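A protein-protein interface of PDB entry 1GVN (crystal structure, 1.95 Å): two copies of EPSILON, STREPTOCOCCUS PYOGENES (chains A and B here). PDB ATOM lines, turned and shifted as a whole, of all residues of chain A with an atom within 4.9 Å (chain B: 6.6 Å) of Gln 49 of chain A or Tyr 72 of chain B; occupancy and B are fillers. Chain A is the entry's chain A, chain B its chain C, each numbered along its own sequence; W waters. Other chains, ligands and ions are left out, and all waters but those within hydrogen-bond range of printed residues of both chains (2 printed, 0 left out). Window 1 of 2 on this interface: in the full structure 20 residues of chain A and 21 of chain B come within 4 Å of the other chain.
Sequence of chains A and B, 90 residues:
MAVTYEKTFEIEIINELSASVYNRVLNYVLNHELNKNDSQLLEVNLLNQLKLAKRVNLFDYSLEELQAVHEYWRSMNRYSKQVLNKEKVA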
ATOM      1  N   ASN A  45       1.289 -22.251  18.806  1.00  0.00           N
ATOM      2  CA  ASN A  45       2.348 -21.874  17.876  1.00  0.00           C
ATOM      3  C   ASN A  45       3.488 -21.275  18.704  1.00  0.00           C
ATOM      4  O   ASN A  45       4.665 -21.582  18.488  1.00  0.00           O
ATOM      5  CB  ASN A  45       1.827 -20.851  16.865  1.00  0.00           C
ATOM      6  CG  ASN A  45       2.862 -20.488  15.815  1.00  0.00           C
ATOM      7  OD1 ASN A  45       3.816 -19.758  16.088  1.00  0.00           O
ATOM      8  ND2 ASN A  45       2.685 -21.010  14.609  1.00  0.00           N
ATOM      9  N   LEU A  46       3.135 -20.437  19.672  1.00  0.00           N
ATOM     10  CA  LEU A  46       4.134 -19.823  20.539  1.00  0.00           C
ATOM     11  C   LEU A  46       4.859 -20.886  21.358  1.00  0.00           C
ATOM     12  O   LEU A  46       6.085 -20.858  21.487  1.00  0.00           O
ATOM     13  CB  LEU A  46       3.476 -18.819  21.489  1.00  0.00           C
ATOM     14  CG  LEU A  46       4.393 -18.219  22.563  1.00  0.00           C
ATOM     15  CD1 LEU A  46       5.559 -17.503  21.907  1.00  0.00           C
ATOM     16  CD2 LEU A  46       3.600 -17.263  23.432  1.00  0.00           C
ATOM     17  N   LEU A  47       4.096 -21.817  21.923  1.00  0.00           N
ATOM     18  CA  LEU A  47       4.681 -22.887  22.718  1.00  0.00           C
ATOM     19  C   LEU A  47       5.725 -23.636  21.891  1.00  0.00           C
ATOM     20  O   LEU A  47       6.825 -23.917  22.367  1.00  0.00           O
ATOM     21  CB  LEU A  47       3.598 -23.872  23.176  1.00  0.00           C
ATOM     22  CG  LEU A  47       4.107 -25.074  23.987  1.00  0.00           C
ATOM     23  CD1 LEU A  47       4.624 -24.602  25.337  1.00  0.00           C
ATOM     24  CD2 LEU A  47       2.984 -26.087  24.187  1.00  0.00           C
ATOM     25  N   ASN A  48       5.371 -23.954  20.649  1.00  0.00           N
ATOM     26  CA  ASN A  48       6.270 -24.682  19.768  1.00  0.00           C
ATOM     27  C   ASN A  48       7.524 -23.894  19.431  1.00  0.00           C
ATOM     28  O   ASN A  48       8.602 -24.469  19.299  1.00  0.00           O
ATOM     29  CB  ASN A  48       5.534 -25.117  18.499  1.00  0.00           C
ATOM     30  CG  ASN A  48       4.509 -26.209  18.781  1.00  0.00           C
ATOM     31  OD1 ASN A  48       4.655 -26.966  19.739  1.00  0.00           O
ATOM     32  ND2 ASN A  48       3.481 -26.301  17.946  1.00  0.00           N
ATOM     33  N   GLN A  49       7.377 -22.578  19.299  1.00  0.00           N
ATOM     34  CA  GLN A  49       8.558 -21.761  19.049  1.00  0.00           C
ATOM     35  C   GLN A  49       9.494 -21.764  20.254  1.00  0.00           C
ATOM     36  O   GLN A  49      10.694 -21.816  20.126  1.00  0.00           O
ATOM     37  CB  GLN A  49       8.156 -20.328  18.698  1.00  0.00           C
ATOM     38  CG  GLN A  49       7.427 -20.195  17.371  1.00  0.00           C
ATOM     39  CD  GLN A  49       7.043 -18.763  17.059  1.00  0.00           C
ATOM     40  OE1 GLN A  49       7.903 -17.889  16.955  1.00  0.00           O
ATOM     41  NE2 GLN A  49       5.747 -18.520  16.905  1.00  0.00           N
ATOM     42  N   LEU A  50       8.865 -21.762  21.435  1.00  0.00           N
ATOM     43  CA  LEU A  50       9.639 -21.788  22.672  1.00  0.00           C
ATOM     44  C   LEU A  50      10.357 -23.129  22.809  1.00  0.00           C
ATOM     45  O   LEU A  50      11.491 -23.185  23.291  1.00  0.00           O
ATOM     46  CB  LEU A  50       8.729 -21.532  23.883  1.00  0.00           C
ATOM     47  CG  LEU A  50       8.011 -20.173  23.945  1.00  0.00           C
ATOM     48  CD1 LEU A  50       7.333 -20.008  25.309  1.00  0.00           C
ATOM     49  CD2 LEU A  50       9.006 -19.044  23.731  1.00  0.00           C
ATOM     50  N   LYS A  51       9.702 -24.208  22.385  1.00  0.00           N
ATOM     51  CA  LYS A  51      10.324 -25.532  22.437  1.00  0.00           C
ATOM     52  C   LYS A  51      11.562 -25.523  21.535  1.00  0.00           C
ATOM     53  O   LYS A  51      12.614 -26.068  21.876  1.00  0.00           O
ATOM     54  CB  LYS A  51       9.345 -26.612  21.949  1.00  0.00           C
ATOM     55  CG  LYS A  51       8.195 -26.904  22.920  1.00  0.00           C
ATOM     56  CD  LYS A  51       7.215 -27.934  22.338  1.00  0.00           C
ATOM     57  CE  LYS A  51       6.204 -28.414  23.384  1.00  0.00           C
ATOM     58  NZ  LYS A  51       6.807 -29.402  24.329  1.00  0.00           N
ATOM     59  N   LEU A  52      11.426 -24.889  20.377  1.00  0.00           N
ATOM     60  CA  LEU A  52      12.524 -24.806  19.422  1.00  0.00           C
ATOM     61  C   LEU A  52      13.675 -24.007  20.037  1.00  0.00           C
ATOM     62  O   LEU A  52      14.847 -24.369  19.910  1.00  0.00           O
ATOM     63  CB  LEU A  52      12.021 -24.143  18.137  1.00  0.00           C
ATOM     64  CG  LEU A  52      12.827 -24.321  16.851  1.00  0.00           C
ATOM     65  CD1 LEU A  52      12.056 -23.718  15.685  1.00  0.00           C
ATOM     66  CD2 LEU A  52      14.183 -23.667  16.996  1.00  0.00           C
ATOM     67  N   ALA A  53      13.334 -22.923  20.717  1.00  0.00           N
ATOM     68  CA  ALA A  53      14.331 -22.073  21.355  1.00  0.00           C
ATOM     69  C   ALA A  53      15.134 -22.830  22.413  1.00  0.00           C
ATOM     70  O   ALA A  53      16.345 -22.645  22.539  1.00  0.00           O
ATOM     71  CB  ALA A  53      13.642 -20.862  21.989  1.00  0.00           C
ATOM     72  N   TYR A  72      16.012 -12.445  23.942  1.00  0.00           N
ATOM     73  CA  TYR A  72      14.941 -13.237  23.340  1.00  0.00           C
ATOM     74  C   TYR A  72      13.917 -13.591  24.413  1.00  0.00           C
ATOM     75  O   TYR A  72      12.711 -13.399  24.239  1.00  0.00           O
ATOM     76  CB  TYR A  72      15.498 -14.536  22.754  1.00  0.00           C
ATOM     77  CG  TYR A  72      14.427 -15.520  22.325  1.00  0.00           C
ATOM     78  CD1 TYR A  72      13.846 -15.441  21.062  1.00  0.00           C
ATOM     79  CD2 TYR A  72      13.970 -16.508  23.200  1.00  0.00           C
ATOM     80  CE1 TYR A  72      12.832 -16.326  20.675  1.00  0.00           C
ATOM     81  CE2 TYR A  72      12.956 -17.397  22.823  1.00  0.00           C
ATOM     82  CZ  TYR A  72      12.394 -17.301  21.563  1.00  0.00           C
ATOM     83  OH  TYR A  72      11.402 -18.185  21.184  1.00  0.00           O
ATOM     84  N   MET A  76      10.023 -12.540  24.872  1.00  0.00           N
ATOM     85  CA  MET A  76       8.958 -13.541  24.926  1.00  0.00           C
ATOM     86  C   MET A  76       8.242 -13.463  26.269  1.00  0.00           C
ATOM     87  O   MET A  76       7.074 -13.843  26.385  1.00  0.00           O
ATOM     88  CB  MET A  76       9.521 -14.949  24.696  1.00  0.00           C
ATOM     89  CG  MET A  76       9.872 -15.224  23.234  1.00  0.00           C
ATOM     90  SD  MET A  76       8.418 -15.030  22.153  1.00  0.00           S
ATOM     91  CE  MET A  76       8.836 -16.100  20.798  1.00  0.00           C
ATOM     92  N   TYR A  79       5.888 -10.646  25.468  1.00  0.00           N
ATOM     93  CA  TYR A  79       4.898 -11.092  24.494  1.00  0.00           C
ATOM     94  C   TYR A  79       3.900 -12.121  25.028  1.00  0.00           C
ATOM     95  O   TYR A  79       2.700 -12.015  24.768  1.00  0.00           O
ATOM     96  CB  TYR A  79       5.600 -11.659  23.257  1.00  0.00           C
ATOM     97  CG  TYR A  79       4.640 -12.177  22.211  1.00  0.00           C
ATOM     98  CD1 TYR A  79       3.772 -11.314  21.539  1.00  0.00           C
ATOM     99  CD2 TYR A  79       4.572 -13.539  21.919  1.00  0.00           C
ATOM    100  CE1 TYR A  79       2.856 -11.801  20.604  1.00  0.00           C
ATOM    101  CE2 TYR A  79       3.666 -14.034  20.992  1.00  0.00           C
ATOM    102  CZ  TYR A  79       2.812 -13.164  20.343  1.00  0.00           C
ATOM    103  OH  TYR A  79       1.884 -13.673  19.474  1.00  0.00           O
ATOM    104  N   LEU B  17       5.002  -6.462   7.365  1.00  0.00           N
ATOM    105  CA  LEU B  17       6.000  -6.476   8.430  1.00  0.00           C
ATOM    106  C   LEU B  17       6.724  -7.813   8.553  1.00  0.00           C
ATOM    107  O   LEU B  17       7.951  -7.847   8.663  1.00  0.00           O
ATOM    108  CB  LEU B  17       5.360  -6.112   9.773  1.00  0.00           C
ATOM    109  CG  LEU B  17       6.306  -6.059  10.981  1.00  0.00           C
ATOM    110  CD1 LEU B  17       7.439  -5.069  10.717  1.00  0.00           C
ATOM    111  CD2 LEU B  17       5.519  -5.642  12.222  1.00  0.00           C
ATOM    112  N   ASN B  45      18.171 -21.007  14.162  1.00  0.00           N
ATOM    113  CA  ASN B  45      17.127 -21.336  15.120  1.00  0.00           C
ATOM    114  C   ASN B  45      16.061 -20.247  15.026  1.00  0.00           C
ATOM    115  O   ASN B  45      14.868 -20.534  15.004  1.00  0.00           O
ATOM    116  CB  ASN B  45      17.720 -21.401  16.528  1.00  0.00           C
ATOM    117  CG  ASN B  45      16.687 -21.730  17.582  1.00  0.00           C
ATOM    118  OD1 ASN B  45      15.843 -20.904  17.919  1.00  0.00           O
ATOM    119  ND2 ASN B  45      16.752 -22.949  18.111  1.00  0.00           N
ATOM    120  N   LEU B  46      16.500 -18.994  14.943  1.00  0.00           N
ATOM    121  CA  LEU B  46      15.560 -17.881  14.824  1.00  0.00           C
ATOM    122  C   LEU B  46      14.775 -18.005  13.515  1.00  0.00           C
ATOM    123  O   LEU B  46      13.552 -17.835  13.492  1.00  0.00           O
ATOM    124  CB  LEU B  46      16.307 -16.544  14.863  1.00  0.00           C
ATOM    125  CG  LEU B  46      15.421 -15.313  14.621  1.00  0.00           C
ATOM    126  CD1 LEU B  46      14.231 -15.336  15.584  1.00  0.00           C
ATOM    127  CD2 LEU B  46      16.237 -14.040  14.808  1.00  0.00           C
ATOM    128  N   ASN B  48      14.035 -20.643  11.852  1.00  0.00           N
ATOM    129  CA  ASN B  48      13.068 -21.728  11.976  1.00  0.00           C
ATOM    130  C   ASN B  48      11.853 -21.323  12.805  1.00  0.00           C
ATOM    131  O   ASN B  48      10.738 -21.759  12.531  1.00  0.00           O
ATOM    132  CB  ASN B  48      13.746 -22.962  12.576  1.00  0.00           C
ATOM    133  CG  ASN B  48      14.714 -23.613  11.605  1.00  0.00           C
ATOM    134  OD1 ASN B  48      15.657 -24.294  12.012  1.00  0.00           O
ATOM    135  ND2 ASN B  48      14.479 -23.414  10.314  1.00  0.00           N
ATOM    136  N   GLN B  49      12.060 -20.487  13.816  1.00  0.00           N
ATOM    137  CA  GLN B  49      10.942 -20.025  14.630  1.00  0.00           C
ATOM    138  C   GLN B  49      10.022 -19.144  13.782  1.00  0.00           C
ATOM    139  O   GLN B  49       8.793 -19.246  13.870  1.00  0.00           O
ATOM    140  CB  GLN B  49      11.441 -19.231  15.838  1.00  0.00           C
ATOM    141  CG  GLN B  49      12.149 -20.064  16.888  1.00  0.00           C
ATOM    142  CD  GLN B  49      12.478 -19.248  18.120  1.00  0.00           C
ATOM    143  OE1 GLN B  49      11.601 -18.610  18.706  1.00  0.00           O
ATOM    144  NE2 GLN B  49      13.741 -19.257  18.517  1.00  0.00           N
ATOM    145  N   LEU B  50      10.625 -18.287  12.957  1.00  0.00           N
ATOM    146  CA  LEU B  50       9.870 -17.389  12.086  1.00  0.00           C
ATOM    147  C   LEU B  50       9.104 -18.192  11.033  1.00  0.00           C
ATOM    148  O   LEU B  50       8.000 -17.818  10.637  1.00  0.00           O
ATOM    149  CB  LEU B  50      10.809 -16.388  11.402  1.00  0.00           C
ATOM    150  CG  LEU B  50      11.622 -15.466  12.328  1.00  0.00           C
ATOM    151  CD1 LEU B  50      12.443 -14.492  11.486  1.00  0.00           C
ATOM    152  CD2 LEU B  50      10.683 -14.698  13.263  1.00  0.00           C
ATOM    153  N   LYS B  51       9.696 -19.288  10.574  1.00  0.00           N
ATOM    154  CA  LYS B  51       9.037 -20.137   9.590  1.00  0.00           C
ATOM    155  C   LYS B  51       7.772 -20.703  10.223  1.00  0.00           C
ATOM    156  O   LYS B  51       6.712 -20.741   9.603  1.00  0.00           O
ATOM    157  CB  LYS B  51       9.962 -21.282   9.152  1.00  0.00           C
ATOM    158  CG  LYS B  51      11.048 -20.878   8.150  1.00  0.00           C
ATOM    159  CD  LYS B  51      11.973 -22.054   7.832  1.00  0.00           C
ATOM    160  CE  LYS B  51      12.982 -21.711   6.732  1.00  0.00           C
ATOM    161  NZ  LYS B  51      12.361 -21.721   5.371  1.00  0.00           N
ATOM    162  N   LEU B  52       7.893 -21.138  11.471  1.00  0.00           N
ATOM    163  CA  LEU B  52       6.761 -21.695  12.203  1.00  0.00           C
ATOM    164  C   LEU B  52       5.685 -20.627  12.401  1.00  0.00           C
ATOM    165  O   LEU B  52       4.496 -20.894  12.254  1.00  0.00           O
ATOM    166  CB  LEU B  52       7.248 -22.227  13.556  1.00  0.00           C
ATOM    167  CG  LEU B  52       6.230 -22.776  14.557  1.00  0.00           C
ATOM    168  CD1 LEU B  52       5.340 -23.834  13.895  1.00  0.00           C
ATOM    169  CD2 LEU B  52       6.993 -23.375  15.740  1.00  0.00           C
ATOM    170  N   ALA B  53       6.109 -19.411  12.722  1.00  0.00           N
ATOM    171  CA  ALA B  53       5.171 -18.311  12.935  1.00  0.00           C
ATOM    172  C   ALA B  53       4.399 -17.955  11.669  1.00  0.00           C
ATOM    173  O   ALA B  53       3.202 -17.653  11.727  1.00  0.00           O
ATOM    174  CB  ALA B  53       5.917 -17.084  13.443  1.00  0.00           C
ATOM    175  N   LYS B  54       5.085 -17.989  10.530  1.00  0.00           N
ATOM    176  CA  LYS B  54       4.478 -17.653   9.237  1.00  0.00           C
ATOM    177  C   LYS B  54       3.521 -18.687   8.648  1.00  0.00           C
ATOM    178  O   LYS B  54       2.646 -18.341   7.858  1.00  0.00           O
ATOM    179  CB  LYS B  54       5.565 -17.391   8.192  1.00  0.00           C
ATOM    180  CG  LYS B  54       6.223 -16.032   8.252  1.00  0.00           C
ATOM    181  CD  LYS B  54       7.312 -15.947   7.187  1.00  0.00           C
ATOM    182  CE  LYS B  54       6.742 -16.243   5.800  1.00  0.00           C
ATOM    183  NZ  LYS B  54       7.796 -16.560   4.801  1.00  0.00           N
ATOM    184  N   GLN B  67      -4.029  -8.703  16.577  1.00  0.00           N
ATOM    185  CA  GLN B  67      -3.255  -7.638  17.197  1.00  0.00           C
ATOM    186  C   GLN B  67      -2.052  -8.265  17.906  1.00  0.00           C
ATOM    187  O   GLN B  67      -0.975  -7.677  17.945  1.00  0.00           O
ATOM    188  CB  GLN B  67      -4.137  -6.842  18.168  1.00  0.00           C
ATOM    189  CG  GLN B  67      -5.316  -6.175  17.451  1.00  0.00           C
ATOM    190  CD  GLN B  67      -6.311  -5.522  18.394  1.00  0.00           C
ATOM    191  OE1 GLN B  67      -6.579  -6.030  19.480  1.00  0.00           O
ATOM    192  NE2 GLN B  67      -6.883  -4.400  17.966  1.00  0.00           N
ATOM    193  N   ALA B  68      -2.231  -9.470  18.443  1.00  0.00           N
ATOM    194  CA  ALA B  68      -1.133 -10.159  19.116  1.00  0.00           C
ATOM    195  C   ALA B  68      -0.061 -10.548  18.092  1.00  0.00           C
ATOM    196  O   ALA B  68       1.127 -10.338  18.325  1.00  0.00           O
ATOM    197  CB  ALA B  68      -1.642 -11.399  19.830  1.00  0.00           C
ATOM    198  N   VAL B  69      -0.485 -11.116  16.966  1.00  0.00           N
ATOM    199  CA  VAL B  69       0.448 -11.521  15.915  1.00  0.00           C
ATOM    200  C   VAL B  69       1.218 -10.298  15.430  1.00  0.00           C
ATOM    201  O   VAL B  69       2.417 -10.363  15.160  1.00  0.00           O
ATOM    202  CB  VAL B  69      -0.300 -12.164  14.718  1.00  0.00           C
ATOM    203  CG1 VAL B  69       0.668 -12.437  13.571  1.00  0.00           C
ATOM    204  CG2 VAL B  69      -0.960 -13.463  15.164  1.00  0.00           C
ATOM    205  N   HIS B  70       0.519  -9.176  15.321  1.00  0.00           N
ATOM    206  CA  HIS B  70       1.146  -7.941  14.887  1.00  0.00           C
ATOM    207  C   HIS B  70       2.254  -7.562  15.879  1.00  0.00           C
ATOM    208  O   HIS B  70       3.349  -7.158  15.478  1.00  0.00           O
ATOM    209  CB  HIS B  70       0.085  -6.841  14.797  1.00  0.00           C
ATOM    210  CG  HIS B  70       0.562  -5.585  14.144  1.00  0.00           C
ATOM    211  ND1 HIS B  70      -0.288  -4.545  13.835  1.00  0.00           N
ATOM    212  CD2 HIS B  70       1.798  -5.188  13.761  1.00  0.00           C
ATOM    213  CE1 HIS B  70       0.405  -3.561  13.290  1.00  0.00           C
ATOM    214  NE2 HIS B  70       1.672  -3.926  13.234  1.00  0.00           N
ATOM    215  N   GLU B  71       1.981  -7.698  17.176  1.00  0.00           N
ATOM    216  CA  GLU B  71       2.999  -7.372  18.179  1.00  0.00           C
ATOM    217  C   GLU B  71       4.134  -8.390  18.113  1.00  0.00           C
ATOM    218  O   GLU B  71       5.298  -8.046  18.320  1.00  0.00           O
ATOM    219  CB  GLU B  71       2.389  -7.339  19.583  1.00  0.00           C
ATOM    220  CG  GLU B  71       3.387  -7.100  20.721  1.00  0.00           C
ATOM    221  CD  GLU B  71       4.279  -5.885  20.508  1.00  0.00           C
ATOM    222  OE1 GLU B  71       3.848  -4.925  19.833  1.00  0.00           O
ATOM    223  OE2 GLU B  71       5.418  -5.881  21.032  1.00  0.00           O
ATOM    224  N   TYR B  72       3.801  -9.641  17.808  1.00  0.00           N
ATOM    225  CA  TYR B  72       4.827 -10.676  17.692  1.00  0.00           C
ATOM    226  C   TYR B  72       5.859 -10.236  16.662  1.00  0.00           C
ATOM    227  O   TYR B  72       7.067 -10.320  16.893  1.00  0.00           O
ATOM    228  CB  TYR B  72       4.220 -12.014  17.238  1.00  0.00           C
ATOM    229  CG  TYR B  72       5.272 -13.028  16.812  1.00  0.00           C
ATOM    230  CD1 TYR B  72       5.900 -13.853  17.746  1.00  0.00           C
ATOM    231  CD2 TYR B  72       5.671 -13.121  15.477  1.00  0.00           C
ATOM    232  CE1 TYR B  72       6.905 -14.752  17.357  1.00  0.00           C
ATOM    233  CE2 TYR B  72       6.668 -14.006  15.082  1.00  0.00           C
ATOM    234  CZ  TYR B  72       7.278 -14.818  16.023  1.00  0.00           C
ATOM    235  OH  TYR B  72       8.249 -15.696  15.618  1.00  0.00           O
ATOM    236  N   TRP B  73       5.382  -9.762  15.516  1.00  0.00           N
ATOM    237  CA  TRP B  73       6.296  -9.339  14.472  1.00  0.00           C
ATOM    238  C   TRP B  73       7.011  -8.038  14.805  1.00  0.00           C
ATOM    239  O   TRP B  73       8.122  -7.816  14.340  1.00  0.00           O
ATOM    240  CB  TRP B  73       5.571  -9.263  13.125  1.00  0.00           C
ATOM    241  CG  TRP B  73       5.232 -10.635  12.602  1.00  0.00           C
ATOM    242  CD1 TRP B  73       4.000 -11.225  12.569  1.00  0.00           C
ATOM    243  CD2 TRP B  73       6.156 -11.610  12.105  1.00  0.00           C
ATOM    244  NE1 TRP B  73       4.101 -12.506  12.082  1.00  0.00           N
ATOM    245  CE2 TRP B  73       5.413 -12.768  11.791  1.00  0.00           C
ATOM    246  CE3 TRP B  73       7.542 -11.618  11.897  1.00  0.00           C
ATOM    247  CZ2 TRP B  73       6.010 -13.926  11.277  1.00  0.00           C
ATOM    248  CZ3 TRP B  73       8.136 -12.769  11.385  1.00  0.00           C
ATOM    249  CH2 TRP B  73       7.368 -13.907  11.081  1.00  0.00           C
ATOM    250  N   ARG B  74       6.391  -7.179  15.611  1.00  0.00           N
ATOM    251  CA  ARG B  74       7.066  -5.945  16.000  1.00  0.00           C
ATOM    252  C   ARG B  74       8.233  -6.365  16.888  1.00  0.00           C
ATOM    253  O   ARG B  74       9.344  -5.847  16.760  1.00  0.00           O
ATOM    254  CB  ARG B  74       6.155  -5.021  16.818  1.00  0.00           C
ATOM    255  CG  ARG B  74       4.957  -4.446  16.080  1.00  0.00           C
ATOM    256  CD  ARG B  74       4.458  -3.185  16.795  1.00  0.00           C
ATOM    257  NE  ARG B  74       3.147  -2.749  16.321  1.00  0.00           N
ATOM    258  CZ  ARG B  74       1.993  -3.205  16.800  1.00  0.00           C
ATOM    259  NH1 ARG B  74       1.984  -4.110  17.774  1.00  0.00           N
ATOM    260  NH2 ARG B  74       0.843  -2.760  16.303  1.00  0.00           N
ATOM    261  N   SER B  75       7.971  -7.313  17.788  1.00  0.00           N
ATOM    262  CA  SER B  75       8.998  -7.795  18.706  1.00  0.00           C
ATOM    263  C   SER B  75      10.127  -8.499  17.964  1.00  0.00           C
ATOM    264  O   SER B  75      11.292  -8.335  18.312  1.00  0.00           O
ATOM    265  CB  SER B  75       8.401  -8.738  19.763  1.00  0.00           C
ATOM    266  OG  SER B  75       8.031  -9.991  19.209  1.00  0.00           O
ATOM    267  N   MET B  76       9.793  -9.286  16.948  1.00  0.00           N
ATOM    268  CA  MET B  76      10.836  -9.968  16.195  1.00  0.00           C
ATOM    269  C   MET B  76      11.584  -8.979  15.300  1.00  0.00           C
ATOM    270  O   MET B  76      12.751  -9.183  14.982  1.00  0.00           O
ATOM    271  CB  MET B  76      10.252 -11.116  15.368  1.00  0.00           C
ATOM    272  CG  MET B  76       9.852 -12.320  16.213  1.00  0.00           C
ATOM    273  SD  MET B  76      11.240 -13.004  17.159  1.00  0.00           S
ATOM    274  CE  MET B  76      10.985 -14.783  16.903  1.00  0.00           C
ATOM    275  N   ASN B  77      10.914  -7.908  14.891  1.00  0.00           N
ATOM    276  CA  ASN B  77      11.574  -6.905  14.068  1.00  0.00           C
ATOM    277  C   ASN B  77      12.695  -6.323  14.934  1.00  0.00           C
ATOM    278  O   ASN B  77      13.848  -6.232  14.504  1.00  0.00           O
ATOM    279  CB  ASN B  77      10.584  -5.811  13.657  1.00  0.00           C
ATOM    280  CG  ASN B  77      11.198  -4.791  12.700  1.00  0.00           C
ATOM    281  OD1 ASN B  77      11.978  -5.142  11.811  1.00  0.00           O
ATOM    282  ND2 ASN B  77      10.832  -3.523  12.875  1.00  0.00           N
HETATM  283  O   HOH W   1      16.296 -25.899  18.098  1.00  0.00           O
HETATM  284  O   HOH W   2       9.087 -11.985  21.816  1.00  0.00           O
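OE1 of Gln 49 of chain A lies within hydrogen-bond range of OH of Tyr 72 of chain B (2.6 Å).
The backbone carbonyl oxygen of Gln 49 of chain B lies close to the side-chain amide oxygen of Gln 49 of chain A (3.5 Å).
The backbone carbonyl oxygen (O) of Leu 52 of chain A lies close to the side-chain amide nitrogen (ND2) of Asn 45 of chain B (3.0 Å).
The side-chain amide nitrogen of Asn 45 of chain A lies within hydrogen-bond range of the backbone carbonyl oxygen of Leu 52 of chain B, 3.0 Å away.
The side-chain amide oxygen (OE1) of Gln 49 of chain B is in hydrogen-bond range of the side-chain hydroxyl (OH) of Tyr 72 of chain A (2.5 Å).
OD1 of Asn 45 of chain B is in hydrogen-bond range of NE2 of Gln 49 of chain B (2.7 Å).
OG of Ser 75 of chain B lies within hydrogen-bond range of O of Tyr 72 of chain B, at 2.5 Å.
NE2 of Gln 49 of chain A lies within hydrogen-bond range of OD1 of Asn 45 of chain A.
Asn 45 of chain A touches Ala 53 of chain B (OD1 to CA, 3.7 Å).
Asn 48 of chain A touches Leu 52 of chain B (CB to CD2, 3.6 Å).
Gln 49 of chain A touches Leu 52 of chain B.
Ala 53 of chain B touches Gln 49 of chain A.
Leu 52 of chain A touches Asn 48 of chain B (CD1 to CB, 3.6 Å).
N of Gln 49 of chain B touches CD1 of Leu 52 of chain A, 3.7 Å away.
CA of Ala 53 of chain A touches OD1 of Asn 45 of chain B, 3.9 Å away.
Gln 49 of chain B touches Ala 53 of chain A.
O of Ala 68 of chain B touches CE1 of Tyr 79 of chain A, 3.2 Å away.
CZ of Tyr 79 of chain A touches CB of Tyr 72 of chain B, at 3.6 Å.
Of the printed residues of chain B, Leu 52 of chain A touches Asn 45, Asn 48 and Gln 49.
Printed residues of chain B within 4 Å of Ala 53 of chain A: Asn 45 (3.9 Å) and Gln 49 (3.8 Å).
Tyr 72 of chain B touches two residues of chain A.
The nearest residue of chain A that does not touch Tyr 72 of chain B is Met 76 of chain A (4.2 Å).
Of the 12 printed residues of chain A, 7 touch a printed residue of chain B.
Printed residues of chain A that touch a printed residue of chain B: Asn 45, Asn 48, Gln 49, Leu 52, Ala 53, Tyr 72 and Tyr 79.
Along chain A the printed residues that touch a printed residue of chain B span positions 45 to 79.
Among the printed residues, no Asp or Glu carboxylate lies within 4 Å of a Lys or Arg side-chain nitrogen of the other chain.
Asn 45 of chain A touches Leu 52 of chain B, and with the chains exchanged Leu 52 of chain A touches Asn 45 of chain B.
Gln 49 of chain A touches Leu 52 of chain B, and with the chains exchanged Leu 52 of chain A touches Gln 49 of chain B.
Gln 49 of chain A touches Ala 53 of chain B, and with the chains exchanged Ala 53 of chain A touches Gln 49 of chain B.
Gln 49 of chain A touches Tyr 72 of chain B, and with the chains exchanged Tyr 72 of chain A touches Gln 49 of chain B.
Of the 15 pairs that touch across the chains among the printed residues, 13 have their exchanged pair printed and touching as well.
Water W1 lies within hydrogen-bond range of O of Leu 52 of chain A (2.8 Å) and ND2 of Asn 45 of chain B (3.0 Å).
Water W2 lies within hydrogen-bond range of SD of Met 76 of chain A (3.1 Å) and OG of Ser 75 of chain B (3.4 Å).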
